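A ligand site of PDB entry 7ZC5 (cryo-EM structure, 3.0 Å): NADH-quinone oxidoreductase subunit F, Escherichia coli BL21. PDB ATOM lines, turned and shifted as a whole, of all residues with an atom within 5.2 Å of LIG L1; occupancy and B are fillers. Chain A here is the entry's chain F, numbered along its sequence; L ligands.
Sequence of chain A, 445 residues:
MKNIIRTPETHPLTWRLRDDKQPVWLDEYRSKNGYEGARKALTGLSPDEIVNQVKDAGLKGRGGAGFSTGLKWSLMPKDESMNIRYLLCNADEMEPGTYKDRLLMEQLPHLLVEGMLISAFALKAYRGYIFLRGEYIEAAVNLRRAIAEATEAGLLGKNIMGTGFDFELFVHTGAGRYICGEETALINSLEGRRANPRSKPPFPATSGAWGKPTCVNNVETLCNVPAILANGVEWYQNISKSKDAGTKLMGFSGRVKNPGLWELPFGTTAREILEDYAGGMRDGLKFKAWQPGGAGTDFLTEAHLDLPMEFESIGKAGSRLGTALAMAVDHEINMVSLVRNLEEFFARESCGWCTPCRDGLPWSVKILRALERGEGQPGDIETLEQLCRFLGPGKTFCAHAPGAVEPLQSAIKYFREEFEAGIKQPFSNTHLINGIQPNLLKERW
ND2 of Asn 90 sits at hydrogen-bond distance from O5 of LIG L1, at 2.6 Å.
The backbone NH of Asn 218 is in hydrogen-bond range of an oxygen (O9) of LIG L1, at 2.6 Å.
An oxygen (O1) of LIG L1 lies close to the side-chain amide oxygen of Asn 218 (2.8 Å).
N of Gly 63 sits at hydrogen-bond distance from O7 of LIG L1, at 3.0 Å.
N of Glu 93 lies within hydrogen-bond range of O2 of LIG L1, 3.0 Å away.
The side-chain amino group of Lys 72 is in salt-bridge range of an oxygen (O8) of LIG L1, 3.2 Å away.
OG1 of Thr 221 sits at hydrogen-bond distance from O9 of LIG L1 (3.4 Å).
ND2 of Asn 217 lies within hydrogen-bond range of O8 of LIG L1 (3.5 Å).
An oxygen (O5) of LG2 L2 sits at hydrogen-bond distance from the side-chain amino group of Lys 72, at 3.1 Å.
OE2 of Glu 183 is in hydrogen-bond range of O6 of LG2 L2.
An oxygen (O12) of LG2 L2 is in hydrogen-bond range of the backbone carbonyl oxygen (O) of Gly 64, 3.0 Å away.
The backbone NH (N) of Ala 65 sits at hydrogen-bond distance from an oxygen (O12) of LG2 L2 (3.3 Å).
N3 of LIG L1 lies close to O of Gly 181.
Gly 61 touches LIG L1 (CA to O8, 3.3 Å).
N of Arg 62 touches O7 of LIG L1, 3.6 Å away.
CB of Asp 92 touches O2 of LIG L1, 3.5 Å away.
Met 94 touches LIG L1.
Tyr 178 touches LIG L1 (CE2 to C7, 3.9 Å).
Ile 179 touches LIG L1 (CD1 to C7, 3.7 Å).
N of Glu 182 touches C4 of LIG L1, 3.5 Å away.
Glu 183 touches LIG L1.
O of Val 216 touches C17 of LIG L1 (3.8 Å).
CB of Ala 399 touches C9 of LIG L1, at 3.7 Å.
His 400 touches LIG L1 (CB to C7, 3.8 Å).
Hydrophobic or aromatic side chains that line LIG L1: Tyr 178, Ile 179, Ala 399 and His 400.
Within 4 Å of LIG L1: Gly 61, Arg 62, Gly 63, Lys 72, Asn 90, Asp 92, Glu 93, Met 94, Tyr 178, Ile 179, Gly 181, Glu 182, Glu 183, Val 216, Asn 217, Asn 218, Thr 221, Ala 399 and His 400.
The side-chain amide nitrogen of Asn 90 sits at hydrogen-bond distance from the backbone carbonyl oxygen of Gly 181.
The backbone NH (N) of Asn 90 sits at hydrogen-bond distance from the backbone carbonyl oxygen (O) of Asn 217, at 2.8 Å.
The side-chain amide nitrogen (ND2) of Asn 218 lies close to the backbone NH (N) of Gly 63, at 3.4 Å.
O of Arg 62 sits at hydrogen-bond distance from ND2 of Asn 218 (2.9 Å).
The side-chain amide oxygen (OD1) of Asn 218 lies close to the side-chain carboxylate (OD2) of Asp 101, 3.4 Å away.
The side-chain carboxylate (OD2) of Asp 92 lies within hydrogen-bond range of the backbone NH (N) of Gly 181, at 2.9 Å.
The side-chain amino group (NZ) of Lys 72 lies close to the side-chain amide nitrogen (ND2) of Asn 217 (3.2 Å).
OG1 of Thr 221 is in hydrogen-bond range of N of Arg 62 (3.4 Å).
An oxygen (O3) of LIG L1 is in hydrogen-bond range of an oxygen (O9) of LG2 L2.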
ATOM      1  N   GLY A  61     -14.529  -5.450 -19.860  1.00  0.00           N
ATOM      2  CA  GLY A  61     -13.116  -5.373 -20.187  1.00  0.00           C
ATOM      3  C   GLY A  61     -12.728  -3.998 -20.681  1.00  0.00           C
ATOM      4  O   GLY A  61     -13.293  -3.484 -21.653  1.00  0.00           O
ATOM      5  N   ARG A  62     -11.744  -3.396 -20.016  1.00  0.00           N
ATOM      6  CA  ARG A  62     -11.264  -2.058 -20.346  1.00  0.00           C
ATOM      7  C   ARG A  62     -10.156  -2.085 -21.376  1.00  0.00           C
ATOM      8  O   ARG A  62      -9.488  -1.061 -21.572  1.00  0.00           O
ATOM      9  CB  ARG A  62     -10.789  -1.342 -19.090  1.00  0.00           C
ATOM     10  CG  ARG A  62     -11.815  -1.270 -17.994  1.00  0.00           C
ATOM     11  CD  ARG A  62     -13.075  -0.619 -18.474  1.00  0.00           C
ATOM     12  NE  ARG A  62     -13.739   0.119 -17.418  1.00  0.00           N
ATOM     13  CZ  ARG A  62     -14.849  -0.275 -16.812  1.00  0.00           C
ATOM     14  NH1 ARG A  62     -15.457  -1.391 -17.165  1.00  0.00           N
ATOM     15  NH2 ARG A  62     -15.349   0.464 -15.837  1.00  0.00           N
ATOM     16  N   GLY A  63      -9.926  -3.216 -22.016  1.00  0.00           N
ATOM     17  CA  GLY A  63      -8.961  -3.327 -23.077  1.00  0.00           C
ATOM     18  C   GLY A  63      -9.505  -2.998 -24.442  1.00  0.00           C
ATOM     19  O   GLY A  63      -8.787  -3.135 -25.432  1.00  0.00           O
ATOM     20  N   GLY A  64     -10.759  -2.559 -24.539  1.00  0.00           N
ATOM     21  CA  GLY A  64     -11.304  -2.150 -25.805  1.00  0.00           C
ATOM     22  C   GLY A  64     -12.521  -2.908 -26.266  1.00  0.00           C
ATOM     23  O   GLY A  64     -13.456  -2.323 -26.823  1.00  0.00           O
ATOM     24  N   ALA A  65     -12.539  -4.223 -26.051  1.00  0.00           N
ATOM     25  CA  ALA A  65     -13.634  -5.028 -26.575  1.00  0.00           C
ATOM     26  C   ALA A  65     -14.875  -4.983 -25.709  1.00  0.00           C
ATOM     27  O   ALA A  65     -15.979  -5.208 -26.202  1.00  0.00           O
ATOM     28  CB  ALA A  65     -13.177  -6.464 -26.764  1.00  0.00           C
ATOM     29  N   GLY A  66     -14.722  -4.701 -24.419  1.00  0.00           N
ATOM     30  CA  GLY A  66     -15.872  -4.559 -23.556  1.00  0.00           C
ATOM     31  C   GLY A  66     -16.528  -5.859 -23.137  1.00  0.00           C
ATOM     32  O   GLY A  66     -17.701  -5.842 -22.758  1.00  0.00           O
ATOM     33  N   PHE A  67     -15.808  -6.970 -23.206  1.00  0.00           N
ATOM     34  CA  PHE A  67     -16.339  -8.230 -22.716  1.00  0.00           C
ATOM     35  C   PHE A  67     -16.427  -8.205 -21.191  1.00  0.00           C
ATOM     36  O   PHE A  67     -15.607  -7.586 -20.515  1.00  0.00           O
ATOM     37  CB  PHE A  67     -15.467  -9.391 -23.173  1.00  0.00           C
ATOM     38  CG  PHE A  67     -16.153 -10.729 -23.161  1.00  0.00           C
ATOM     39  CD1 PHE A  67     -17.042 -11.061 -24.167  1.00  0.00           C
ATOM     40  CD2 PHE A  67     -15.915 -11.634 -22.153  1.00  0.00           C
ATOM     41  CE1 PHE A  67     -17.673 -12.284 -24.164  1.00  0.00           C
ATOM     42  CE2 PHE A  67     -16.554 -12.861 -22.146  1.00  0.00           C
ATOM     43  CZ  PHE A  67     -17.437 -13.180 -23.153  1.00  0.00           C
ATOM     44  N   THR A  69     -15.959  -9.198 -17.478  1.00  0.00           N
ATOM     45  CA  THR A  69     -14.861  -9.857 -16.793  1.00  0.00           C
ATOM     46  C   THR A  69     -15.346 -11.003 -15.916  1.00  0.00           C
ATOM     47  O   THR A  69     -14.634 -12.005 -15.772  1.00  0.00           O
ATOM     48  CB  THR A  69     -14.085  -8.835 -15.968  1.00  0.00           C
ATOM     49  OG1 THR A  69     -13.865  -7.675 -16.775  1.00  0.00           O
ATOM     50  CG2 THR A  69     -12.755  -9.376 -15.535  1.00  0.00           C
ATOM     51  N   LYS A  72     -15.879 -13.910 -18.219  1.00  0.00           N
ATOM     52  CA  LYS A  72     -14.582 -14.472 -18.578  1.00  0.00           C
ATOM     53  C   LYS A  72     -13.995 -15.290 -17.448  1.00  0.00           C
ATOM     54  O   LYS A  72     -13.370 -16.330 -17.681  1.00  0.00           O
ATOM     55  CB  LYS A  72     -13.618 -13.347 -18.975  1.00  0.00           C
ATOM     56  CG  LYS A  72     -13.147 -13.426 -20.389  1.00  0.00           C
ATOM     57  CD  LYS A  72     -12.359 -12.201 -20.772  1.00  0.00           C
ATOM     58  CE  LYS A  72     -11.046 -12.175 -20.065  1.00  0.00           C
ATOM     59  NZ  LYS A  72     -10.213 -11.069 -20.588  1.00  0.00           N
ATOM     60  N   ASN A  90      -2.365  -7.725 -19.497  1.00  0.00           N
ATOM     61  CA  ASN A  90      -2.028  -7.222 -20.814  1.00  0.00           C
ATOM     62  C   ASN A  90      -1.613  -5.767 -20.687  1.00  0.00           C
ATOM     63  O   ASN A  90      -2.393  -4.834 -20.912  1.00  0.00           O
ATOM     64  CB  ASN A  90      -3.219  -7.389 -21.759  1.00  0.00           C
ATOM     65  CG  ASN A  90      -2.833  -7.305 -23.208  1.00  0.00           C
ATOM     66  OD1 ASN A  90      -1.858  -6.654 -23.573  1.00  0.00           O
ATOM     67  ND2 ASN A  90      -3.602  -7.964 -24.058  1.00  0.00           N
ATOM     68  N   ASP A  92       0.628  -4.471 -22.617  1.00  0.00           N
ATOM     69  CA  ASP A  92       1.310  -4.125 -23.859  1.00  0.00           C
ATOM     70  C   ASP A  92       0.967  -2.702 -24.276  1.00  0.00           C
ATOM     71  O   ASP A  92       1.848  -1.837 -24.326  1.00  0.00           O
ATOM     72  CB  ASP A  92       0.949  -5.110 -24.965  1.00  0.00           C
ATOM     73  CG  ASP A  92       2.090  -5.299 -25.961  1.00  0.00           C
ATOM     74  OD1 ASP A  92       3.254  -5.181 -25.552  1.00  0.00           O
ATOM     75  OD2 ASP A  92       1.807  -5.541 -27.145  1.00  0.00           O
ATOM     76  N   GLU A  93      -0.305  -2.444 -24.558  1.00  0.00           N
ATOM     77  CA  GLU A  93      -0.842  -1.116 -24.870  1.00  0.00           C
ATOM     78  C   GLU A  93      -0.069  -0.443 -26.005  1.00  0.00           C
ATOM     79  O   GLU A  93       0.595   0.577 -25.819  1.00  0.00           O
ATOM     80  CB  GLU A  93      -0.867  -0.226 -23.621  1.00  0.00           C
ATOM     81  CG  GLU A  93      -1.866   0.893 -23.714  1.00  0.00           C
ATOM     82  CD  GLU A  93      -1.497   2.065 -22.844  1.00  0.00           C
ATOM     83  OE1 GLU A  93      -0.300   2.433 -22.811  1.00  0.00           O
ATOM     84  OE2 GLU A  93      -2.398   2.613 -22.196  1.00  0.00           O
ATOM     85  N   MET A  94      -0.146  -1.057 -27.172  1.00  0.00           N
ATOM     86  CA  MET A  94       0.601  -0.585 -28.314  1.00  0.00           C
ATOM     87  C   MET A  94      -0.248   0.231 -29.279  1.00  0.00           C
ATOM     88  O   MET A  94       0.255   0.655 -30.320  1.00  0.00           O
ATOM     89  CB  MET A  94       1.211  -1.771 -29.056  1.00  0.00           C
ATOM     90  CG  MET A  94       2.565  -2.225 -28.580  1.00  0.00           C
ATOM     91  SD  MET A  94       3.869  -1.651 -29.661  1.00  0.00           S
ATOM     92  CE  MET A  94       5.266  -1.869 -28.586  1.00  0.00           C
ATOM     93  N   GLU A  95      -1.516   0.445 -28.968  1.00  0.00           N
ATOM     94  CA  GLU A  95      -2.399   1.146 -29.887  1.00  0.00           C
ATOM     95  C   GLU A  95      -2.041   2.620 -29.942  1.00  0.00           C
ATOM     96  O   GLU A  95      -1.890   3.253 -28.888  1.00  0.00           O
ATOM     97  CB  GLU A  95      -3.858   0.980 -29.474  1.00  0.00           C
ATOM     98  CG  GLU A  95      -4.878   1.621 -30.396  1.00  0.00           C
ATOM     99  CD  GLU A  95      -5.404   0.664 -31.464  1.00  0.00           C
ATOM    100  OE1 GLU A  95      -4.606  -0.075 -32.074  1.00  0.00           O
ATOM    101  OE2 GLU A  95      -6.635   0.641 -31.685  1.00  0.00           O
ATOM    102  N   ASP A 101      -2.542   3.023 -19.605  1.00  0.00           N
ATOM    103  CA  ASP A 101      -1.836   2.043 -18.795  1.00  0.00           C
ATOM    104  C   ASP A 101      -0.499   2.581 -18.302  1.00  0.00           C
ATOM    105  O   ASP A 101      -0.069   2.228 -17.202  1.00  0.00           O
ATOM    106  CB  ASP A 101      -1.627   0.745 -19.576  1.00  0.00           C
ATOM    107  CG  ASP A 101      -2.916   0.146 -20.056  1.00  0.00           C
ATOM    108  OD1 ASP A 101      -3.986   0.527 -19.543  1.00  0.00           O
ATOM    109  OD2 ASP A 101      -2.864  -0.733 -20.943  1.00  0.00           O
ATOM    110  N   TYR A 178       3.216  -4.808 -31.979  1.00  0.00           N
ATOM    111  CA  TYR A 178       1.850  -4.412 -31.651  1.00  0.00           C
ATOM    112  C   TYR A 178       0.942  -5.610 -31.503  1.00  0.00           C
ATOM    113  O   TYR A 178       0.034  -5.616 -30.665  1.00  0.00           O
ATOM    114  CB  TYR A 178       1.332  -3.467 -32.735  1.00  0.00           C
ATOM    115  CG  TYR A 178      -0.157  -3.217 -32.760  1.00  0.00           C
ATOM    116  CD1 TYR A 178      -0.751  -2.360 -31.851  1.00  0.00           C
ATOM    117  CD2 TYR A 178      -0.961  -3.804 -33.718  1.00  0.00           C
ATOM    118  CE1 TYR A 178      -2.091  -2.119 -31.885  1.00  0.00           C
ATOM    119  CE2 TYR A 178      -2.301  -3.563 -33.752  1.00  0.00           C
ATOM    120  CZ  TYR A 178      -2.864  -2.722 -32.844  1.00  0.00           C
ATOM    121  OH  TYR A 178      -4.210  -2.478 -32.887  1.00  0.00           O
ATOM    122  N   ILE A 179       1.176  -6.654 -32.300  1.00  0.00           N
ATOM    123  CA  ILE A 179       0.357  -7.857 -32.281  1.00  0.00           C
ATOM    124  C   ILE A 179       0.504  -8.630 -30.971  1.00  0.00           C
ATOM    125  O   ILE A 179      -0.355  -9.450 -30.646  1.00  0.00           O
ATOM    126  CB  ILE A 179       0.682  -8.723 -33.515  1.00  0.00           C
ATOM    127  CG1 ILE A 179      -0.434  -9.726 -33.810  1.00  0.00           C
ATOM    128  CG2 ILE A 179       2.007  -9.424 -33.336  1.00  0.00           C
ATOM    129  CD1 ILE A 179      -1.808  -9.152 -33.733  1.00  0.00           C
ATOM    130  N   GLY A 181      -0.086  -7.554 -28.135  1.00  0.00           N
ATOM    131  CA  GLY A 181      -1.186  -7.230 -27.261  1.00  0.00           C
ATOM    132  C   GLY A 181      -2.415  -8.077 -27.458  1.00  0.00           C
ATOM    133  O   GLY A 181      -3.258  -8.140 -26.556  1.00  0.00           O
ATOM    134  N   GLU A 182      -2.546  -8.712 -28.628  1.00  0.00           N
ATOM    135  CA  GLU A 182      -3.584  -9.707 -28.851  1.00  0.00           C
ATOM    136  C   GLU A 182      -3.402 -10.847 -27.864  1.00  0.00           C
ATOM    137  O   GLU A 182      -2.290 -11.362 -27.708  1.00  0.00           O
ATOM    138  CB  GLU A 182      -3.503 -10.237 -30.274  1.00  0.00           C
ATOM    139  CG  GLU A 182      -4.810 -10.399 -30.970  1.00  0.00           C
ATOM    140  CD  GLU A 182      -5.542 -11.652 -30.598  1.00  0.00           C
ATOM    141  OE1 GLU A 182      -5.036 -12.750 -30.886  1.00  0.00           O
ATOM    142  OE2 GLU A 182      -6.647 -11.565 -30.034  1.00  0.00           O
ATOM    143  N   GLU A 183      -4.487 -11.247 -27.201  1.00  0.00           N
ATOM    144  CA  GLU A 183      -4.370 -12.087 -26.013  1.00  0.00           C
ATOM    145  C   GLU A 183      -3.809 -13.466 -26.339  1.00  0.00           C
ATOM    146  O   GLU A 183      -2.943 -13.972 -25.609  1.00  0.00           O
ATOM    147  CB  GLU A 183      -5.716 -12.219 -25.306  1.00  0.00           C
ATOM    148  CG  GLU A 183      -6.859 -12.555 -26.217  1.00  0.00           C
ATOM    149  CD  GLU A 183      -7.895 -13.391 -25.514  1.00  0.00           C
ATOM    150  OE1 GLU A 183      -7.947 -13.345 -24.263  1.00  0.00           O
ATOM    151  OE2 GLU A 183      -8.659 -14.093 -26.202  1.00  0.00           O
ATOM    152  N   VAL A 216      -6.463 -13.614 -19.495  1.00  0.00           N
ATOM    153  CA  VAL A 216      -5.808 -12.383 -19.906  1.00  0.00           C
ATOM    154  C   VAL A 216      -6.762 -11.230 -19.631  1.00  0.00           C
ATOM    155  O   VAL A 216      -7.906 -11.236 -20.088  1.00  0.00           O
ATOM    156  CB  VAL A 216      -5.428 -12.417 -21.393  1.00  0.00           C
ATOM    157  CG1 VAL A 216      -4.607 -11.205 -21.753  1.00  0.00           C
ATOM    158  CG2 VAL A 216      -4.664 -13.680 -21.711  1.00  0.00           C
ATOM    159  N   ASN A 217      -6.300 -10.243 -18.851  1.00  0.00           N
ATOM    160  CA  ASN A 217      -7.106  -9.065 -18.563  1.00  0.00           C
ATOM    161  C   ASN A 217      -6.230  -7.838 -18.718  1.00  0.00           C
ATOM    162  O   ASN A 217      -5.017  -7.904 -18.533  1.00  0.00           O
ATOM    163  CB  ASN A 217      -7.705  -9.106 -17.163  1.00  0.00           C
ATOM    164  CG  ASN A 217      -8.991  -9.895 -17.101  1.00  0.00           C
ATOM    165  OD1 ASN A 217      -9.066 -10.916 -16.426  1.00  0.00           O
ATOM    166  ND2 ASN A 217     -10.003  -9.428 -17.810  1.00  0.00           N
ATOM    167  N   ASN A 218      -6.857  -6.711 -19.042  1.00  0.00           N
ATOM    168  CA  ASN A 218      -6.145  -5.464 -19.224  1.00  0.00           C
ATOM    169  C   ASN A 218      -5.670  -4.929 -17.876  1.00  0.00           C
ATOM    170  O   ASN A 218      -6.071  -5.408 -16.810  1.00  0.00           O
ATOM    171  CB  ASN A 218      -7.043  -4.438 -19.922  1.00  0.00           C
ATOM    172  CG  ASN A 218      -6.276  -3.256 -20.477  1.00  0.00           C
ATOM    173  OD1 ASN A 218      -5.080  -3.344 -20.727  1.00  0.00           O
ATOM    174  ND2 ASN A 218      -6.965  -2.150 -20.648  1.00  0.00           N
ATOM    175  N   THR A 221      -8.784  -3.059 -16.104  1.00  0.00           N
ATOM    176  CA  THR A 221      -9.765  -3.945 -15.493  1.00  0.00           C
ATOM    177  C   THR A 221      -9.308  -4.428 -14.118  1.00  0.00           C
ATOM    178  O   THR A 221     -10.055  -4.364 -13.127  1.00  0.00           O
ATOM    179  CB  THR A 221     -10.028  -5.132 -16.407  1.00  0.00           C
ATOM    180  OG1 THR A 221      -9.675  -4.780 -17.749  1.00  0.00           O
ATOM    181  CG2 THR A 221     -11.477  -5.509 -16.384  1.00  0.00           C
ATOM    182  N   CYS A 398      -7.175 -12.868 -37.186  1.00  0.00           N
ATOM    183  CA  CYS A 398      -7.439 -12.141 -35.956  1.00  0.00           C
ATOM    184  C   CYS A 398      -8.054 -10.775 -36.265  1.00  0.00           C
ATOM    185  O   CYS A 398      -8.390 -10.503 -37.416  1.00  0.00           O
ATOM    186  CB  CYS A 398      -6.160 -11.994 -35.131  1.00  0.00           C
ATOM    187  SG  CYS A 398      -5.197 -10.506 -35.421  1.00  0.00           S
ATOM    188  N   ALA A 399      -8.218  -9.927 -35.254  1.00  0.00           N
ATOM    189  CA  ALA A 399      -8.924  -8.671 -35.424  1.00  0.00           C
ATOM    190  C   ALA A 399      -7.985  -7.494 -35.638  1.00  0.00           C
ATOM    191  O   ALA A 399      -8.355  -6.352 -35.363  1.00  0.00           O
ATOM    192  CB  ALA A 399      -9.833  -8.418 -34.227  1.00  0.00           C
ATOM    193  N   HIS A 400      -6.769  -7.746 -36.123  1.00  0.00           N
ATOM    194  CA  HIS A 400      -5.874  -6.653 -36.453  1.00  0.00           C
ATOM    195  C   HIS A 400      -6.321  -5.920 -37.707  1.00  0.00           C
ATOM    196  O   HIS A 400      -6.327  -4.687 -37.736  1.00  0.00           O
ATOM    197  CB  HIS A 400      -4.459  -7.185 -36.638  1.00  0.00           C
ATOM    198  CG  HIS A 400      -3.475  -6.182 -37.157  1.00  0.00           C
ATOM    199  ND1 HIS A 400      -2.749  -5.356 -36.334  1.00  0.00           N
ATOM    200  CD2 HIS A 400      -3.080  -5.898 -38.421  1.00  0.00           C
ATOM    201  CE1 HIS A 400      -1.958  -4.602 -37.069  1.00  0.00           C
ATOM    202  NE2 HIS A 400      -2.136  -4.910 -38.335  1.00  0.00           N
HETATM  203  N1  LIG L   1      -5.550  -5.436 -25.242  1.00  0.00           N
HETATM  204  C1  LIG L   1      -4.705  -4.810 -24.355  1.00  0.00           C
HETATM  205  O1  LIG L   1      -5.064  -4.704 -23.192  1.00  0.00           O
HETATM  206  N2  LIG L   1      -3.503  -4.310 -24.773  1.00  0.00           N
HETATM  207  C2  LIG L   1      -3.135  -4.451 -26.090  1.00  0.00           C
HETATM  208  O2  LIG L   1      -2.060  -4.005 -26.467  1.00  0.00           O
HETATM  209  C3  LIG L   1      -3.972  -5.072 -26.982  1.00  0.00           C
HETATM  210  N3  LIG L   1      -3.599  -5.205 -28.287  1.00  0.00           N
HETATM  211  C4  LIG L   1      -4.423  -5.840 -29.168  1.00  0.00           C
HETATM  212  C5  LIG L   1      -4.026  -5.962 -30.488  1.00  0.00           C
HETATM  213  C6  LIG L   1      -4.851  -6.584 -31.401  1.00  0.00           C
HETATM  214  C7  LIG L   1      -4.411  -6.712 -32.818  1.00  0.00           C
HETATM  215  C8  LIG L   1      -6.067  -7.085 -30.987  1.00  0.00           C
HETATM  216  C9  LIG L   1      -6.972  -7.761 -31.969  1.00  0.00           C
HETATM  217  C10 LIG L   1      -6.469  -6.976 -29.665  1.00  0.00           C
HETATM  218  C11 LIG L   1      -5.646  -6.345 -28.748  1.00  0.00           C
HETATM  219  N4  LIG L   1      -6.022  -6.209 -27.426  1.00  0.00           N
HETATM  220  C12 LIG L   1      -5.181  -5.576 -26.559  1.00  0.00           C
HETATM  221  C13 LIG L   1      -7.326  -6.744 -26.893  1.00  0.00           C
HETATM  222  C14 LIG L   1      -7.091  -8.140 -26.302  1.00  0.00           C
HETATM  223  O3  LIG L   1      -7.319  -9.099 -27.296  1.00  0.00           O
HETATM  224  C15 LIG L   1      -8.003  -8.452 -25.123  1.00  0.00           C
HETATM  225  O4  LIG L   1      -9.311  -8.073 -25.475  1.00  0.00           O
HETATM  226  C16 LIG L   1      -7.567  -7.696 -23.879  1.00  0.00           C
HETATM  227  O5  LIG L   1      -6.170  -7.604 -23.849  1.00  0.00           O
HETATM  228  C17 LIG L   1      -8.033  -8.320 -22.575  1.00  0.00           C
HETATM  229  O6  LIG L   1      -9.434  -8.272 -22.464  1.00  0.00           O
HETATM  230  P1  LIG L   1     -10.123  -7.309 -21.382  1.00  0.00           P
HETATM  231  O7  LIG L   1     -10.602  -6.101 -22.122  1.00  0.00           O
HETATM  232  O8  LIG L   1     -11.271  -8.000 -20.712  1.00  0.00           O
HETATM  233  O9  LIG L   1      -9.126  -6.900 -20.346  1.00  0.00           O
HETATM  234  P1  LG2 L   2     -12.722 -10.106 -28.600  1.00  0.00           P
HETATM  235  O1  LG2 L   2     -13.979  -9.400 -28.891  1.00  0.00           O
HETATM  236  O2  LG2 L   2     -12.407 -11.277 -29.502  1.00  0.00           O
HETATM  237  O3  LG2 L   2     -12.715 -10.655 -27.104  1.00  0.00           O
HETATM  238  C1  LG2 L   2     -12.261  -9.849 -25.999  1.00  0.00           C
HETATM  239  C2  LG2 L   2     -12.023 -10.681 -24.770  1.00  0.00           C
HETATM  240  O4  LG2 L   2     -13.197 -11.462 -24.458  1.00  0.00           O
HETATM  241  C3  LG2 L   2     -10.859 -11.656 -24.835  1.00  0.00           C
HETATM  242  O5  LG2 L   2     -10.208 -11.762 -23.580  1.00  0.00           O
HETATM  243  C4  LG2 L   2     -11.546 -12.973 -25.221  1.00  0.00           C
HETATM  244  O6  LG2 L   2     -10.828 -14.098 -24.748  1.00  0.00           O
HETATM  245  C5  LG2 L   2     -12.888 -12.845 -24.500  1.00  0.00           C
HETATM  246  N1  LG2 L   2     -13.982 -13.529 -25.157  1.00  0.00           N
HETATM  247  C6  LG2 L   2     -14.766 -13.040 -26.178  1.00  0.00           C
HETATM  248  N2  LG2 L   2     -15.696 -13.873 -26.577  1.00  0.00           N
HETATM  249  C7  LG2 L   2     -15.505 -14.993 -25.768  1.00  0.00           C
HETATM  250  C8  LG2 L   2     -16.165 -16.229 -25.697  1.00  0.00           C
HETATM  251  N3  LG2 L   2     -17.207 -16.569 -26.467  1.00  0.00           N
HETATM  252  N4  LG2 L   2     -15.721 -17.123 -24.799  1.00  0.00           N
HETATM  253  C9  LG2 L   2     -14.679 -16.798 -24.020  1.00  0.00           C
HETATM  254  N5  LG2 L   2     -13.992 -15.662 -23.997  1.00  0.00           N
HETATM  255  C10 LG2 L   2     -14.453 -14.790 -24.901  1.00  0.00           C
HETATM  256  O7  LG2 L   2     -11.468  -9.133 -28.616  1.00  0.00           O
HETATM  257  P2  LG2 L   2     -10.114  -9.065 -29.460  1.00  0.00           P
HETATM  258  O8  LG2 L   2     -10.493  -9.308 -30.904  1.00  0.00           O
HETATM  259  O9  LG2 L   2      -9.074  -9.952 -28.919  1.00  0.00           O
HETATM  260  O10 LG2 L   2      -9.645  -7.545 -29.381  1.00  0.00           O
HETATM  261  C11 LG2 L   2     -10.180  -6.499 -30.212  1.00  0.00           C
HETATM  262  C12 LG2 L   2     -10.452  -5.303 -29.323  1.00  0.00           C
HETATM  263  O11 LG2 L   2      -9.205  -4.856 -28.736  1.00  0.00           O
HETATM  264  C13 LG2 L   2     -11.080  -4.091 -30.016  1.00  0.00           C
HETATM  265  O12 LG2 L   2     -12.184  -3.588 -29.282  1.00  0.00           O
HETATM  266  C14 LG2 L   2      -9.935  -3.076 -30.056  1.00  0.00           C
HETATM  267  O13 LG2 L   2     -10.424  -1.745 -29.896  1.00  0.00           O
HETATM  268  C15 LG2 L   2      -9.122  -3.458 -28.825  1.00  0.00           C
HETATM  269  N6  LG2 L   2      -7.716  -3.093 -28.947  1.00  0.00           N
HETATM  270  C16 LG2 L   2      -7.048  -2.493 -27.874  1.00  0.00           C
HETATM  271  C17 LG2 L   2      -5.750  -2.133 -27.930  1.00  0.00           C
HETATM  272  C18 LG2 L   2      -5.164  -1.529 -26.720  1.00  0.00           C
HETATM  273  O14 LG2 L   2      -5.832  -1.398 -25.693  1.00  0.00           O
HETATM  274  N7  LG2 L   2      -3.899  -1.131 -26.780  1.00  0.00           N
HETATM  275  C19 LG2 L   2      -4.948  -2.378 -29.173  1.00  0.00           C
HETATM  276  C20 LG2 L   2      -5.761  -2.988 -30.244  1.00  0.00           C
HETATM  277  C21 LG2 L   2      -7.032  -3.313 -30.097  1.00  0.00           C
